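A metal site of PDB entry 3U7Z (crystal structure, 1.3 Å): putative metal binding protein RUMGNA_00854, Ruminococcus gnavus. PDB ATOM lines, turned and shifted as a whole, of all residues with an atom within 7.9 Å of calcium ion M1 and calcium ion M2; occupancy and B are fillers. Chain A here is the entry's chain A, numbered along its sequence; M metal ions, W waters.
O of Thr 55 is in hydrogen-bond range of N of Asp 43 (2.9 Å).
Four residues have an atom within 4 Å of calcium ion M1: Glu 37, Asn 40, Val 42 and Asp 43. Along chain A the residues within 4 Å of calcium ion M1 span positions 37 to 43. The nearest printed residue that does not touch calcium ion M1 is Gly 44 (5.1 Å).
OD1 of Asn 40 is bound to calcium ion M1 (2.4 Å). Calcium ion M1 is bound by the backbone carbonyl oxygen (O) of Val 42, 2.4 Å away. OD1 of Asp 43 binds calcium ion M1 (2.4 Å). OE1 of Glu 37 binds calcium ion M1 (2.5 Å). The side-chain carboxylate (OE2) of Glu 37 binds calcium ion M1 (2.5 Å). Calcium ion M1 has five donor atoms within binding distance.
Calcium ion M2 is bound by water W1 (2.4 Å). Calcium ion M2 is bound by OD2 of Asp 43 (2.5 Å). Water W2 is bound to calcium ion M2, 2.5 Å away. OD1 of Asp 43 is bound to calcium ion M2 (2.6 Å).
One residue has an atom within 4 Å of calcium ion M2: Asp 43.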
ATOM      1  N   LEU A  36     -25.232  -2.599  15.121  1.00  0.00           N
ATOM      2  CA  LEU A  36     -24.436  -2.473  16.347  1.00  0.00           C
ATOM      3  C   LEU A  36     -24.342  -1.011  16.768  1.00  0.00           C
ATOM      4  O   LEU A  36     -24.480  -0.642  17.981  1.00  0.00           O
ATOM      5  CB  LEU A  36     -23.062  -3.040  16.093  1.00  0.00           C
ATOM      6  CG  LEU A  36     -22.967  -4.540  15.756  1.00  0.00           C
ATOM      7  CD1 LEU A  36     -21.548  -5.002  15.343  1.00  0.00           C
ATOM      8  CD2 LEU A  36     -23.497  -5.357  16.912  1.00  0.00           C
ATOM      9  N   GLU A  37     -24.165  -0.131  15.776  1.00  0.00           N
ATOM     10  CA  GLU A  37     -23.973   1.299  16.082  1.00  0.00           C
ATOM     11  C   GLU A  37     -25.273   2.019  16.373  1.00  0.00           C
ATOM     12  O   GLU A  37     -25.222   3.074  16.988  1.00  0.00           O
ATOM     13  CB  GLU A  37     -23.152   2.049  15.024  1.00  0.00           C
ATOM     14  CG  GLU A  37     -21.667   1.729  15.152  1.00  0.00           C
ATOM     15  CD  GLU A  37     -20.977   2.388  16.364  1.00  0.00           C
ATOM     16  OE1 GLU A  37     -21.646   2.845  17.335  1.00  0.00           O
ATOM     17  OE2 GLU A  37     -19.743   2.479  16.350  1.00  0.00           O
ATOM     18  N   SER A  38     -26.420   1.384  16.101  1.00  0.00           N
ATOM     19  CA  SER A  38     -27.705   2.009  16.355  1.00  0.00           C
ATOM     20  C   SER A  38     -27.893   2.361  17.800  1.00  0.00           C
ATOM     21  O   SER A  38     -28.568   3.353  18.120  1.00  0.00           O
ATOM     22  CB  SER A  38     -28.859   1.177  15.786  1.00  0.00           C
ATOM     23  OG  SER A  38     -29.070  -0.026  16.476  1.00  0.00           O
ATOM     24  N   GLU A  39     -27.304   1.545  18.682  1.00  0.00           N
ATOM     25  CA  GLU A  39     -27.359   1.709  20.118  1.00  0.00           C
ATOM     26  C   GLU A  39     -25.972   2.009  20.695  1.00  0.00           C
ATOM     27  O   GLU A  39     -25.771   1.882  21.901  1.00  0.00           O
ATOM     28  CB  GLU A  39     -27.912   0.427  20.759  1.00  0.00           C
ATOM     29  CG  GLU A  39     -29.344   0.080  20.383  1.00  0.00           C
ATOM     30  CD  GLU A  39     -30.353   1.025  21.020  1.00  0.00           C
ATOM     31  OE1 GLU A  39     -30.088   1.529  22.132  1.00  0.00           O
ATOM     32  OE2 GLU A  39     -31.401   1.270  20.402  1.00  0.00           O
ATOM     33  N   ASN A  40     -25.009   2.366  19.843  1.00  0.00           N
ATOM     34  CA  ASN A  40     -23.646   2.530  20.271  1.00  0.00           C
ATOM     35  C   ASN A  40     -23.119   1.328  21.086  1.00  0.00           C
ATOM     36  O   ASN A  40     -22.464   1.486  22.100  1.00  0.00           O
ATOM     37  CB  ASN A  40     -23.433   3.867  20.974  1.00  0.00           C
ATOM     38  CG  ASN A  40     -21.991   4.247  21.048  1.00  0.00           C
ATOM     39  OD1 ASN A  40     -21.154   3.684  20.367  1.00  0.00           O
ATOM     40  ND2 ASN A  40     -21.680   5.179  21.875  1.00  0.00           N
ATOM     41  N   LEU A  41     -23.360   0.136  20.583  1.00  0.00           N
ATOM     42  CA  LEU A  41     -22.913  -1.085  21.281  1.00  0.00           C
ATOM     43  C   LEU A  41     -21.440  -1.406  21.046  1.00  0.00           C
ATOM     44  O   LEU A  41     -20.865  -2.169  21.769  1.00  0.00           O
ATOM     45  CB  LEU A  41     -23.773  -2.276  20.853  1.00  0.00           C
ATOM     46  CG  LEU A  41     -23.538  -3.649  21.526  1.00  0.00           C
ATOM     47  CD1 LEU A  41     -23.803  -3.535  23.039  1.00  0.00           C
ATOM     48  CD2 LEU A  41     -24.419  -4.687  20.849  1.00  0.00           C
ATOM     49  N   VAL A  42     -20.855  -0.804  20.019  1.00  0.00           N
ATOM     50  CA  VAL A  42     -19.464  -0.989  19.682  1.00  0.00           C
ATOM     51  C   VAL A  42     -18.810   0.332  19.374  1.00  0.00           C
ATOM     52  O   VAL A  42     -19.483   1.341  19.099  1.00  0.00           O
ATOM     53  CB  VAL A  42     -19.300  -1.882  18.447  1.00  0.00           C
ATOM     54  CG1 VAL A  42     -19.989  -3.288  18.619  1.00  0.00           C
ATOM     55  CG2 VAL A  42     -19.767  -1.216  17.176  1.00  0.00           C
ATOM     56  N   ASP A  43     -17.488   0.353  19.468  1.00  0.00           N
ATOM     57  CA  ASP A  43     -16.665   1.414  18.874  1.00  0.00           C
ATOM     58  C   ASP A  43     -15.695   0.732  17.942  1.00  0.00           C
ATOM     59  O   ASP A  43     -15.106  -0.313  18.269  1.00  0.00           O
ATOM     60  CB  ASP A  43     -15.905   2.219  19.917  1.00  0.00           C
ATOM     61  CG  ASP A  43     -16.646   3.401  20.461  1.00  0.00           C
ATOM     62  OD1 ASP A  43     -17.789   3.690  20.122  1.00  0.00           O
ATOM     63  OD2 ASP A  43     -15.974   4.081  21.291  1.00  0.00           O
ATOM     64  N   GLY A  44     -15.530   1.332  16.760  1.00  0.00           N
ATOM     65  CA  GLY A  44     -14.590   0.860  15.826  1.00  0.00           C
ATOM     66  C   GLY A  44     -13.965   1.940  15.018  1.00  0.00           C
ATOM     67  O   GLY A  44     -14.453   3.052  14.983  1.00  0.00           O
ATOM     68  N   LEU A  51     -14.487  -2.120   9.100  1.00  0.00           N
ATOM     69  CA  LEU A  51     -14.441  -1.688  10.464  1.00  0.00           C
ATOM     70  C   LEU A  51     -13.595  -2.597  11.334  1.00  0.00           C
ATOM     71  O   LEU A  51     -13.756  -3.833  11.268  1.00  0.00           O
ATOM     72  CB  LEU A  51     -15.886  -1.664  10.991  1.00  0.00           C
ATOM     73  CG  LEU A  51     -16.118  -1.058  12.375  1.00  0.00           C
ATOM     74  CD1 LEU A  51     -15.678   0.415  12.419  1.00  0.00           C
ATOM     75  CD2 LEU A  51     -17.601  -1.210  12.820  1.00  0.00           C
ATOM     76  N   THR A  55     -13.979  -1.955  20.862  1.00  0.00           N
ATOM     77  CA  THR A  55     -14.758  -1.955  22.086  1.00  0.00           C
ATOM     78  C   THR A  55     -16.132  -2.488  21.785  1.00  0.00           C
ATOM     79  O   THR A  55     -16.760  -2.063  20.808  1.00  0.00           O
ATOM     80  CB  THR A  55     -14.882  -0.547  22.698  1.00  0.00           C
ATOM     81  OG1 THR A  55     -13.593  -0.030  22.925  1.00  0.00           O
ATOM     82  CG2 THR A  55     -15.701  -0.509  24.003  1.00  0.00           C
HETATM   83 CA    CA M   1     -19.629   3.666  18.577  1.00  0.00          CA
HETATM   84 CA    CA M   2     -17.213   6.145  20.747  1.00  0.00          CA
HETATM   85  O   HOH W   1     -15.320   6.916  22.039  1.00  0.00           O
HETATM   86  O   HOH W   2     -18.765   6.857  22.540  1.00  0.00           O
